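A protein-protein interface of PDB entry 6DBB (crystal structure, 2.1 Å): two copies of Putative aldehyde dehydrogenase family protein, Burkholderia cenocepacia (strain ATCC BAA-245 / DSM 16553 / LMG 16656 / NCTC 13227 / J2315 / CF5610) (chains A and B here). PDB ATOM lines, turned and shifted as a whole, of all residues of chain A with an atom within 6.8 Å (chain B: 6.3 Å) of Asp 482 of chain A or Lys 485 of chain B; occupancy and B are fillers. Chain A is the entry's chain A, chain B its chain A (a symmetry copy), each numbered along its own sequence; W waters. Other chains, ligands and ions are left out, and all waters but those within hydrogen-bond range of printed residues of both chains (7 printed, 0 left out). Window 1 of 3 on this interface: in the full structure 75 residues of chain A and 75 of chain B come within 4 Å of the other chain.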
ATOM      1  N   PHE A 120       0.615  -4.210   8.635  1.00  0.00           N
ATOM      2  CA  PHE A 120       0.780  -5.282   7.660  1.00  0.00           C
ATOM      3  C   PHE A 120       2.152  -5.916   7.786  1.00  0.00           C
ATOM      4  O   PHE A 120       2.285  -7.146   7.789  1.00  0.00           O
ATOM      5  CB  PHE A 120       0.552  -4.744   6.246  1.00  0.00           C
ATOM      6  CG  PHE A 120       0.705  -5.788   5.179  1.00  0.00           C
ATOM      7  CD1 PHE A 120      -0.260  -6.780   5.016  1.00  0.00           C
ATOM      8  CD2 PHE A 120       1.797  -5.776   4.333  1.00  0.00           C
ATOM      9  CE1 PHE A 120      -0.133  -7.750   4.021  1.00  0.00           C
ATOM     10  CE2 PHE A 120       1.933  -6.747   3.333  1.00  0.00           C
ATOM     11  CZ  PHE A 120       0.969  -7.727   3.174  1.00  0.00           C
ATOM     12  N   LEU A 124       3.686  -9.741   8.440  1.00  0.00           N
ATOM     13  CA  LEU A 124       4.736 -10.373   7.652  1.00  0.00           C
ATOM     14  C   LEU A 124       5.907 -10.822   8.518  1.00  0.00           C
ATOM     15  O   LEU A 124       6.615 -11.769   8.152  1.00  0.00           O
ATOM     16  CB  LEU A 124       5.245  -9.409   6.572  1.00  0.00           C
ATOM     17  CG  LEU A 124       4.368  -9.022   5.387  1.00  0.00           C
ATOM     18  CD1 LEU A 124       5.131  -8.013   4.516  1.00  0.00           C
ATOM     19  CD2 LEU A 124       4.018 -10.266   4.578  1.00  0.00           C
ATOM     20  N   LEU A 171       8.687  -2.712   5.317  1.00  0.00           N
ATOM     21  CA  LEU A 171       9.060  -4.020   4.782  1.00  0.00           C
ATOM     22  C   LEU A 171      10.551  -4.277   4.948  1.00  0.00           C
ATOM     23  O   LEU A 171      10.955  -5.352   5.411  1.00  0.00           O
ATOM     24  CB  LEU A 171       8.667  -4.119   3.306  1.00  0.00           C
ATOM     25  CG  LEU A 171       7.289  -4.738   3.017  1.00  0.00           C
ATOM     26  CD1 LEU A 171       6.214  -4.029   3.757  1.00  0.00           C
ATOM     27  CD2 LEU A 171       6.996  -4.740   1.513  1.00  0.00           C
ATOM     28  N   GLY A 464      -2.846  -4.446   0.775  1.00  0.00           N
ATOM     29  CA  GLY A 464      -2.702  -5.886   0.580  1.00  0.00           C
ATOM     30  C   GLY A 464      -2.279  -6.304  -0.829  1.00  0.00           C
ATOM     31  O   GLY A 464      -1.861  -7.451  -1.022  1.00  0.00           O
ATOM     32  N   ALA A 466       0.024  -5.954  -4.442  1.00  0.00           N
ATOM     33  CA  ALA A 466       1.300  -5.464  -4.945  1.00  0.00           C
ATOM     34  C   ALA A 466       1.053  -4.210  -5.776  1.00  0.00           C
ATOM     35  O   ALA A 466       0.135  -4.167  -6.607  1.00  0.00           O
ATOM     36  CB  ALA A 466       2.004  -6.530  -5.782  1.00  0.00           C
ATOM     37  N   ARG A 477       7.480  -3.645  -7.728  1.00  0.00           N
ATOM     38  CA  ARG A 477       6.265  -3.777  -6.930  1.00  0.00           C
ATOM     39  C   ARG A 477       6.575  -3.445  -5.479  1.00  0.00           C
ATOM     40  O   ARG A 477       7.621  -3.837  -4.958  1.00  0.00           O
ATOM     41  CB  ARG A 477       5.654  -5.196  -7.013  1.00  0.00           C
ATOM     42  CG  ARG A 477       5.072  -5.589  -8.389  1.00  0.00           C
ATOM     43  CD  ARG A 477       3.915  -4.693  -8.819  1.00  0.00           C
ATOM     44  NE  ARG A 477       3.289  -5.148 -10.062  1.00  0.00           N
ATOM     45  CZ  ARG A 477       3.746  -4.874 -11.281  1.00  0.00           C
ATOM     46  NH1 ARG A 477       4.846  -4.130 -11.434  1.00  0.00           N
ATOM     47  NH2 ARG A 477       3.103  -5.332 -12.349  1.00  0.00           N
ATOM     48  N   SER A 479       4.672  -2.964  -1.340  1.00  0.00           N
ATOM     49  CA  SER A 479       3.591  -3.168  -0.378  1.00  0.00           C
ATOM     50  C   SER A 479       3.116  -4.620  -0.279  1.00  0.00           C
ATOM     51  O   SER A 479       3.734  -5.417   0.431  1.00  0.00           O
ATOM     52  CB  SER A 479       2.423  -2.234  -0.694  1.00  0.00           C
ATOM     53  OG  SER A 479       1.462  -2.264   0.344  1.00  0.00           O
ATOM     54  N   GLY A 480       2.029  -4.978  -0.962  1.00  0.00           N
ATOM     55  CA  GLY A 480       1.287  -6.188  -0.654  1.00  0.00           C
ATOM     56  C   GLY A 480       1.761  -7.423  -1.404  1.00  0.00           C
ATOM     57  O   GLY A 480       2.808  -7.439  -2.054  1.00  0.00           O
ATOM     58  N   SER A 481       0.951  -8.487  -1.297  1.00  0.00           N
ATOM     59  CA  SER A 481       1.297  -9.787  -1.864  1.00  0.00           C
ATOM     60  C   SER A 481       2.696 -10.191  -1.425  1.00  0.00           C
ATOM     61  O   SER A 481       3.047  -9.996  -0.257  1.00  0.00           O
ATOM     62  CB  SER A 481       1.201  -9.771  -3.391  1.00  0.00           C
ATOM     63  OG  SER A 481       1.456 -11.066  -3.892  1.00  0.00           O
ATOM     64  N   ASP A 482       3.523 -10.724  -2.334  1.00  0.00           N
ATOM     65  CA  ASP A 482       4.892 -11.077  -1.971  1.00  0.00           C
ATOM     66  C   ASP A 482       5.912 -10.039  -2.438  1.00  0.00           C
ATOM     67  O   ASP A 482       7.078 -10.376  -2.682  1.00  0.00           O
ATOM     68  CB  ASP A 482       5.270 -12.479  -2.469  1.00  0.00           C
ATOM     69  CG  ASP A 482       5.246 -12.624  -3.990  1.00  0.00           C
ATOM     70  OD1 ASP A 482       4.754 -11.730  -4.702  1.00  0.00           O
ATOM     71  OD2 ASP A 482       5.738 -13.666  -4.482  1.00  0.00           O
ATOM     72  N   ALA A 483       5.514  -8.764  -2.491  1.00  0.00           N
ATOM     73  CA  ALA A 483       6.466  -7.695  -2.798  1.00  0.00           C
ATOM     74  C   ALA A 483       7.662  -7.703  -1.847  1.00  0.00           C
ATOM     75  O   ALA A 483       8.770  -7.293  -2.235  1.00  0.00           O
ATOM     76  CB  ALA A 483       5.757  -6.334  -2.754  1.00  0.00           C
ATOM     77  N   TRP A 484       7.460  -8.183  -0.611  1.00  0.00           N
ATOM     78  CA  TRP A 484       8.531  -8.222   0.385  1.00  0.00           C
ATOM     79  C   TRP A 484       9.777  -8.966  -0.108  1.00  0.00           C
ATOM     80  O   TRP A 484      10.883  -8.688   0.366  1.00  0.00           O
ATOM     81  CB  TRP A 484       8.021  -8.867   1.693  1.00  0.00           C
ATOM     82  CG  TRP A 484       7.583 -10.320   1.546  1.00  0.00           C
ATOM     83  CD1 TRP A 484       6.308 -10.780   1.347  1.00  0.00           C
ATOM     84  CD2 TRP A 484       8.423 -11.493   1.609  1.00  0.00           C
ATOM     85  NE1 TRP A 484       6.307 -12.154   1.264  1.00  0.00           N
ATOM     86  CE2 TRP A 484       7.587 -12.617   1.434  1.00  0.00           C
ATOM     87  CE3 TRP A 484       9.795 -11.698   1.808  1.00  0.00           C
ATOM     88  CZ2 TRP A 484       8.082 -13.928   1.423  1.00  0.00           C
ATOM     89  CZ3 TRP A 484      10.289 -12.996   1.798  1.00  0.00           C
ATOM     90  CH2 TRP A 484       9.433 -14.096   1.603  1.00  0.00           C
ATOM     91  N   LYS A 485       9.628  -9.908  -1.048  1.00  0.00           N
ATOM     92  CA  LYS A 485      10.786 -10.670  -1.532  1.00  0.00           C
ATOM     93  C   LYS A 485      11.840  -9.778  -2.167  1.00  0.00           C
ATOM     94  O   LYS A 485      13.021 -10.139  -2.194  1.00  0.00           O
ATOM     95  CB  LYS A 485      10.349 -11.736  -2.548  1.00  0.00           C
ATOM     96  CG  LYS A 485       9.669 -12.955  -1.889  1.00  0.00           C
ATOM     97  CD  LYS A 485       8.973 -13.832  -2.913  1.00  0.00           C
ATOM     98  CE  LYS A 485       8.232 -14.983  -2.185  1.00  0.00           C
ATOM     99  NZ  LYS A 485       7.418 -15.773  -3.156  1.00  0.00           N
ATOM    100  N   ALA A 486      11.444  -8.615  -2.680  1.00  0.00           N
ATOM    101  CA  ALA A 486      12.428  -7.711  -3.275  1.00  0.00           C
ATOM    102  C   ALA A 486      13.367  -7.095  -2.242  1.00  0.00           C
ATOM    103  O   ALA A 486      14.354  -6.465  -2.632  1.00  0.00           O
ATOM    104  CB  ALA A 486      11.724  -6.602  -4.058  1.00  0.00           C
ATOM    105  N   TYR B 129      -0.032 -19.811 -10.349  1.00  0.00           N
ATOM    106  CA  TYR B 129      -0.873 -19.294  -9.276  1.00  0.00           C
ATOM    107  C   TYR B 129      -0.629 -17.811  -9.014  1.00  0.00           C
ATOM    108  O   TYR B 129       0.495 -17.390  -8.738  1.00  0.00           O
ATOM    109  CB  TYR B 129      -0.582 -20.057  -7.989  1.00  0.00           C
ATOM    110  CG  TYR B 129      -1.011 -21.518  -7.967  1.00  0.00           C
ATOM    111  CD1 TYR B 129      -2.212 -21.934  -8.551  1.00  0.00           C
ATOM    112  CD2 TYR B 129      -0.218 -22.480  -7.343  1.00  0.00           C
ATOM    113  CE1 TYR B 129      -2.612 -23.267  -8.497  1.00  0.00           C
ATOM    114  CE2 TYR B 129      -0.616 -23.823  -7.296  1.00  0.00           C
ATOM    115  CZ  TYR B 129      -1.809 -24.204  -7.882  1.00  0.00           C
ATOM    116  OH  TYR B 129      -2.219 -25.529  -7.837  1.00  0.00           O
ATOM    117  N   LEU B 131      -3.141 -14.912  -6.571  1.00  0.00           N
ATOM    118  CA  LEU B 131      -3.790 -14.897  -5.272  1.00  0.00           C
ATOM    119  C   LEU B 131      -5.176 -14.301  -5.412  1.00  0.00           C
ATOM    120  O   LEU B 131      -5.410 -13.431  -6.253  1.00  0.00           O
ATOM    121  CB  LEU B 131      -3.001 -14.063  -4.243  1.00  0.00           C
ATOM    122  CG  LEU B 131      -1.565 -14.498  -3.957  1.00  0.00           C
ATOM    123  CD1 LEU B 131      -0.839 -13.423  -3.121  1.00  0.00           C
ATOM    124  CD2 LEU B 131      -1.544 -15.877  -3.251  1.00  0.00           C
ATOM    125  N   GLU B 144      -4.869 -11.103  -7.538  1.00  0.00           N
ATOM    126  CA  GLU B 144      -3.633 -10.905  -8.277  1.00  0.00           C
ATOM    127  C   GLU B 144      -3.587 -11.975  -9.359  1.00  0.00           C
ATOM    128  O   GLU B 144      -3.685 -13.168  -9.052  1.00  0.00           O
ATOM    129  CB  GLU B 144      -2.425 -11.001  -7.339  1.00  0.00           C
ATOM    130  CG  GLU B 144      -1.105 -11.184  -8.053  1.00  0.00           C
ATOM    131  CD  GLU B 144       0.044 -11.382  -7.077  1.00  0.00           C
ATOM    132  OE1 GLU B 144       0.409 -10.395  -6.400  1.00  0.00           O
ATOM    133  OE2 GLU B 144       0.555 -12.525  -6.970  1.00  0.00           O
ATOM    134  N   TRP B 146      -1.732 -13.388 -13.191  1.00  0.00           N
ATOM    135  CA  TRP B 146      -0.482 -13.429 -13.929  1.00  0.00           C
ATOM    136  C   TRP B 146      -0.785 -13.611 -15.408  1.00  0.00           C
ATOM    137  O   TRP B 146      -1.687 -14.377 -15.765  1.00  0.00           O
ATOM    138  CB  TRP B 146       0.419 -14.552 -13.420  1.00  0.00           C
ATOM    139  CG  TRP B 146       0.946 -14.251 -12.067  1.00  0.00           C
ATOM    140  CD1 TRP B 146       0.386 -14.591 -10.855  1.00  0.00           C
ATOM    141  CD2 TRP B 146       2.121 -13.502 -11.770  1.00  0.00           C
ATOM    142  NE1 TRP B 146       1.161 -14.107  -9.825  1.00  0.00           N
ATOM    143  CE2 TRP B 146       2.236 -13.440 -10.359  1.00  0.00           C
ATOM    144  CE3 TRP B 146       3.100 -12.889 -12.559  1.00  0.00           C
ATOM    145  CZ2 TRP B 146       3.284 -12.779  -9.728  1.00  0.00           C
ATOM    146  CZ3 TRP B 146       4.150 -12.247 -11.928  1.00  0.00           C
ATOM    147  CH2 TRP B 146       4.228 -12.190 -10.523  1.00  0.00           C
ATOM    148  N   CYS B 175       3.989 -20.429 -20.003  1.00  0.00           N
ATOM    149  CA  CYS B 175       3.533 -19.130 -19.535  1.00  0.00           C
ATOM    150  C   CYS B 175       2.953 -18.261 -20.651  1.00  0.00           C
ATOM    151  O   CYS B 175       2.678 -17.087 -20.402  1.00  0.00           O
ATOM    152  CB  CYS B 175       4.681 -18.386 -18.858  1.00  0.00           C
ATOM    153  SG  CYS B 175       5.191 -19.146 -17.298  1.00  0.00           S
ATOM    154  N   ARG B 262      13.065  -6.305 -18.627  1.00  0.00           N
ATOM    155  CA  ARG B 262      13.376  -7.213 -17.540  1.00  0.00           C
ATOM    156  C   ARG B 262      14.500  -8.163 -17.935  1.00  0.00           C
ATOM    157  O   ARG B 262      14.521  -8.683 -19.056  1.00  0.00           O
ATOM    158  CB  ARG B 262      12.132  -8.007 -17.149  1.00  0.00           C
ATOM    159  CG  ARG B 262      12.378  -8.978 -16.001  1.00  0.00           C
ATOM    160  CD  ARG B 262      11.188  -9.893 -15.817  1.00  0.00           C
ATOM    161  NE  ARG B 262       9.986  -9.139 -15.472  1.00  0.00           N
ATOM    162  CZ  ARG B 262       8.759  -9.650 -15.520  1.00  0.00           C
ATOM    163  NH1 ARG B 262       8.569 -10.913 -15.916  1.00  0.00           N
ATOM    164  NH2 ARG B 262       7.726  -8.899 -15.171  1.00  0.00           N
ATOM    165  N   ASP B 482       9.017 -20.548  -7.682  1.00  0.00           N
ATOM    166  CA  ASP B 482       8.215 -19.634  -8.491  1.00  0.00           C
ATOM    167  C   ASP B 482       9.057 -18.836  -9.485  1.00  0.00           C
ATOM    168  O   ASP B 482       8.682 -17.718  -9.863  1.00  0.00           O
ATOM    169  CB  ASP B 482       7.363 -18.701  -7.621  1.00  0.00           C
ATOM    170  CG  ASP B 482       8.181 -17.773  -6.722  1.00  0.00           C
ATOM    171  OD1 ASP B 482       9.406 -17.943  -6.586  1.00  0.00           O
ATOM    172  OD2 ASP B 482       7.572 -16.845  -6.139  1.00  0.00           O
ATOM    173  N   ALA B 483      10.151 -19.424  -9.980  1.00  0.00           N
ATOM    174  CA  ALA B 483      10.934 -18.780 -11.035  1.00  0.00           C
ATOM    175  C   ALA B 483      10.080 -18.437 -12.254  1.00  0.00           C
ATOM    176  O   ALA B 483      10.375 -17.462 -12.968  1.00  0.00           O
ATOM    177  CB  ALA B 483      12.106 -19.685 -11.443  1.00  0.00           C
ATOM    178  N   TRP B 484       9.010 -19.210 -12.491  1.00  0.00           N
ATOM    179  CA  TRP B 484       8.133 -18.980 -13.640  1.00  0.00           C
ATOM    180  C   TRP B 484       7.580 -17.552 -13.692  1.00  0.00           C
ATOM    181  O   TRP B 484       7.253 -17.062 -14.777  1.00  0.00           O
ATOM    182  CB  TRP B 484       6.964 -19.991 -13.629  1.00  0.00           C
ATOM    183  CG  TRP B 484       6.046 -19.876 -12.418  1.00  0.00           C
ATOM    184  CD1 TRP B 484       6.107 -20.615 -11.265  1.00  0.00           C
ATOM    185  CD2 TRP B 484       4.923 -18.983 -12.258  1.00  0.00           C
ATOM    186  NE1 TRP B 484       5.111 -20.225 -10.399  1.00  0.00           N
ATOM    187  CE2 TRP B 484       4.363 -19.236 -10.987  1.00  0.00           C
ATOM    188  CE3 TRP B 484       4.333 -18.006 -13.073  1.00  0.00           C
ATOM    189  CZ2 TRP B 484       3.258 -18.527 -10.498  1.00  0.00           C
ATOM    190  CZ3 TRP B 484       3.239 -17.301 -12.589  1.00  0.00           C
ATOM    191  CH2 TRP B 484       2.713 -17.563 -11.310  1.00  0.00           C
ATOM    192  N   LYS B 485       7.467 -16.869 -12.545  1.00  0.00           N
ATOM    193  CA  LYS B 485       6.917 -15.508 -12.538  1.00  0.00           C
ATOM    194  C   LYS B 485       7.741 -14.547 -13.378  1.00  0.00           C
ATOM    195  O   LYS B 485       7.213 -13.541 -13.865  1.00  0.00           O
ATOM    196  CB  LYS B 485       6.820 -14.969 -11.104  1.00  0.00           C
ATOM    197  CG  LYS B 485       5.647 -15.578 -10.307  1.00  0.00           C
ATOM    198  CD  LYS B 485       5.758 -15.278  -8.824  1.00  0.00           C
ATOM    199  CE  LYS B 485       4.608 -15.992  -8.067  1.00  0.00           C
ATOM    200  NZ  LYS B 485       4.780 -15.834  -6.592  1.00  0.00           N
ATOM    201  N   ALA B 486       9.027 -14.830 -13.565  1.00  0.00           N
ATOM    202  CA  ALA B 486       9.853 -13.950 -14.391  1.00  0.00           C
ATOM    203  C   ALA B 486       9.481 -14.005 -15.870  1.00  0.00           C
ATOM    204  O   ALA B 486       9.974 -13.176 -16.641  1.00  0.00           O
ATOM    205  CB  ALA B 486      11.334 -14.292 -14.217  1.00  0.00           C
ATOM    206  N   TYR B 487       8.621 -14.935 -16.287  1.00  0.00           N
ATOM    207  CA  TYR B 487       8.175 -15.007 -17.677  1.00  0.00           C
ATOM    208  C   TYR B 487       6.778 -14.422 -17.863  1.00  0.00           C
ATOM    209  O   TYR B 487       6.202 -14.523 -18.952  1.00  0.00           O
ATOM    210  CB  TYR B 487       8.235 -16.457 -18.177  1.00  0.00           C
ATOM    211  CG  TYR B 487       9.630 -17.050 -18.016  1.00  0.00           C
ATOM    212  CD1 TYR B 487      10.575 -16.979 -19.047  1.00  0.00           C
ATOM    213  CD2 TYR B 487      10.016 -17.637 -16.816  1.00  0.00           C
ATOM    214  CE1 TYR B 487      11.860 -17.531 -18.889  1.00  0.00           C
ATOM    215  CE2 TYR B 487      11.295 -18.172 -16.641  1.00  0.00           C
ATOM    216  CZ  TYR B 487      12.208 -18.123 -17.669  1.00  0.00           C
ATOM    217  OH  TYR B 487      13.463 -18.654 -17.445  1.00  0.00           O
ATOM    218  N   MET B 488       6.223 -13.814 -16.821  1.00  0.00           N
ATOM    219  CA  MET B 488       4.872 -13.289 -16.867  1.00  0.00           C
ATOM    220  C   MET B 488       4.853 -11.917 -16.199  1.00  0.00           C
ATOM    221  O   MET B 488       5.806 -11.517 -15.523  1.00  0.00           O
ATOM    222  CB  MET B 488       3.889 -14.268 -16.178  1.00  0.00           C
ATOM    223  CG  MET B 488       3.864 -15.667 -16.793  1.00  0.00           C
ATOM    224  SD  MET B 488       2.582 -16.760 -16.152  1.00  0.00           S
ATOM    225  CE  MET B 488       1.180 -16.253 -17.176  1.00  0.00           C
ATOM    226  N   ARG B 489       3.748 -11.195 -16.361  1.00  0.00           N
ATOM    227  CA  ARG B 489       3.587  -9.899 -15.714  1.00  0.00           C
ATOM    228  C   ARG B 489       2.457  -9.966 -14.692  1.00  0.00           C
ATOM    229  O   ARG B 489       1.394 -10.525 -14.964  1.00  0.00           O
ATOM    230  CB  ARG B 489       3.307  -8.777 -16.734  1.00  0.00           C
ATOM    231  CG  ARG B 489       2.067  -8.956 -17.614  1.00  0.00           C
ATOM    232  CD  ARG B 489       1.822  -7.726 -18.539  1.00  0.00           C
ATOM    233  NE  ARG B 489       0.788  -8.019 -19.537  1.00  0.00           N
ATOM    234  CZ  ARG B 489      -0.520  -8.020 -19.292  1.00  0.00           C
ATOM    235  NH1 ARG B 489      -0.981  -7.728 -18.079  1.00  0.00           N
ATOM    236  NH2 ARG B 489      -1.376  -8.323 -20.260  1.00  0.00           N
ATOM    237  N   ARG B 490       2.698  -9.405 -13.513  1.00  0.00           N
ATOM    238  CA  ARG B 490       1.701  -9.393 -12.449  1.00  0.00           C
ATOM    239  C   ARG B 490       0.668  -8.286 -12.660  1.00  0.00           C
ATOM    240  O   ARG B 490       1.012  -7.154 -13.007  1.00  0.00           O
ATOM    241  CB  ARG B 490       2.404  -9.193 -11.102  1.00  0.00           C
ATOM    242  CG  ARG B 490       1.528  -9.367  -9.869  1.00  0.00           C
ATOM    243  CD  ARG B 490       2.184  -8.682  -8.649  1.00  0.00           C
ATOM    244  NE  ARG B 490       3.563  -9.102  -8.429  1.00  0.00           N
ATOM    245  CZ  ARG B 490       3.995  -9.819  -7.394  1.00  0.00           C
ATOM    246  NH1 ARG B 490       3.158 -10.223  -6.430  1.00  0.00           N
ATOM    247  NH2 ARG B 490       5.286 -10.145  -7.330  1.00  0.00           N
HETATM  248  O   HOH W   1       9.127 -18.116  -3.529  1.00  0.00           O
HETATM  249  O   HOH W   2       2.832 -13.728  -6.031  1.00  0.00           O
HETATM  250  O   HOH W   3      -1.114  -8.149  -5.893  1.00  0.00           O
HETATM  251  O   HOH W   4       8.109 -10.538  -5.325  1.00  0.00           O
HETATM  252  O   HOH W   5       4.629 -17.254  -3.720  1.00  0.00           O
HETATM  253  O   HOH W   6       0.525  -5.934  -9.984  1.00  0.00           O
HETATM  254  O   HOH W   7       7.294 -12.700  -6.548  1.00  0.00           O
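Asp 482 of chain A touches Lys 485 of chain B, and with the chains exchanged Lys 485 of chain A touches Asp 482 of chain B.
Hydrophobic or aromatic side chains of chain A that line the printed part of chain B: Ala 466.
Along chain A the printed residues that touch a printed residue of chain B span positions 466 to 485.
Of the 15 printed residues of chain B, 5 touch a printed residue of chain A.
Along chain B the printed residues that touch a printed residue of chain A span positions 131 to 490.
Among the printed residues, 8 pairs touch across the chains.
Among the printed residues, Asp or Glu carboxylates within 4 Å of a Lys or Arg side-chain nitrogen of the other chain: Asp 482 of chain A with Lys 485 of chain B, Asp 482 of chain A with Arg 490 of chain B and Lys 485 of chain A with Asp 482 of chain B.
CD of Arg 490 of chain B touches CB of Ala 466 of chain A, 3.6 Å away.
Ser 481 of chain A touches Leu 131 of chain B.
The guanidinium group (NH2) of Arg 477 of chain A lies within hydrogen-bond range of the backbone carbonyl oxygen (O) of Arg 490 of chain B (2.9 Å).
The side-chain hydroxyl of Ser 481 of chain A is in hydrogen-bond range of the side-chain carboxylate of Glu 144 of chain B (2.8 Å).
The side-chain hydroxyl (OG) of Ser 481 of chain A lies within hydrogen-bond range of the guanidinium group (NH1) of Arg 490 of chain B.
OD2 of Asp 482 of chain A lies within salt-bridge range of NZ of Lys 485 of chain B.
NH1 of Arg 490 of chain B lies within salt-bridge range of OD1 of Asp 482 of chain A (2.8 Å).
NZ of Lys 485 of chain A lies within salt-bridge range of OD2 of Asp 482 of chain B, at 3.2 Å.
The backbone carbonyl oxygen (O) of Gly 464 of chain A is in hydrogen-bond range of the backbone NH (N) of Ser 481 of chain A, at 3.0 Å.
The side-chain carboxylate (OD1) of Asp 482 of chain A is in hydrogen-bond range of the side-chain hydroxyl (OG) of Ser 481 of chain A, at 3.5 Å.
The side-chain amino group of Lys 485 of chain A lies within salt-bridge range of the side-chain carboxylate of Asp 482 of chain A (3.0 Å).
NE1 of Trp 146 of chain B lies within hydrogen-bond range of OE2 of Glu 144 of chain B (3.3 Å).
The guanidinium group of Arg 490 of chain B is in salt-bridge range of the side-chain carboxylate of Glu 144 of chain B (2.8 Å).
OD2 of Asp 482 of chain B lies within salt-bridge range of NZ of Lys 485 of chain B.
Water W3 lies within hydrogen-bond range of the side-chain carboxylate (OE1) of Glu 144 of chain B and the backbone NH (N) of Ala 466 of chain A.
Water W7 lies within hydrogen-bond range of OD2 of Asp 482 of chain A (2.8 Å) and NH2 of Arg 490 of chain B (3.3 Å).
Water W4 bridges O of Asp 482 of chain A (2.8 Å) and NH2 of Arg 490 of chain B (3.5 Å).
Water W6 bridges NE of Arg 477 of chain A (2.9 Å) and O of Arg 490 of chain B (3.3 Å).
Water W1 bridges NZ of Lys 485 of chain A (2.9 Å) and OD1 of Asp 482 of chain B (3.1 Å).
Water W5 bridges NZ of Lys 485 of chain A (3.2 Å) and NZ of Lys 485 of chain B (3.2 Å).
Of chain B, only Lys 485 (3.2 Å) and Arg 490 (2.8 Å) come within 4 Å of Asp 482 of chain A.
Lys 485 of chain B touches just one residue of chain A: Asp 482.
Of the printed residues of chain A, Asp 482 of chain B touches Lys 485 (3.2 Å).
Of the printed residues of chain A, Leu 131 of chain B touches Ser 481 (3.4 Å).
Printed residues of chain B within 4 Å of Lys 485 of chain A: Asp 482 (3.2 Å).
Of the printed residues of chain A, Glu 144 of chain B touches Ser 481 (2.8 Å).
Of the printed residues of chain B, Ser 481 of chain A touches Leu 131, Glu 144 and Arg 490.
Leu 124 of chain A touches none of the printed residues of chain B.
The nearest residue of chain A that does not touch Lys 485 of chain B is Lys 485 of chain A (4.3 Å).
The nearest printed residue of chain B that does not touch Ser 481 of chain A is Trp 146 of chain B (6.4 Å).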
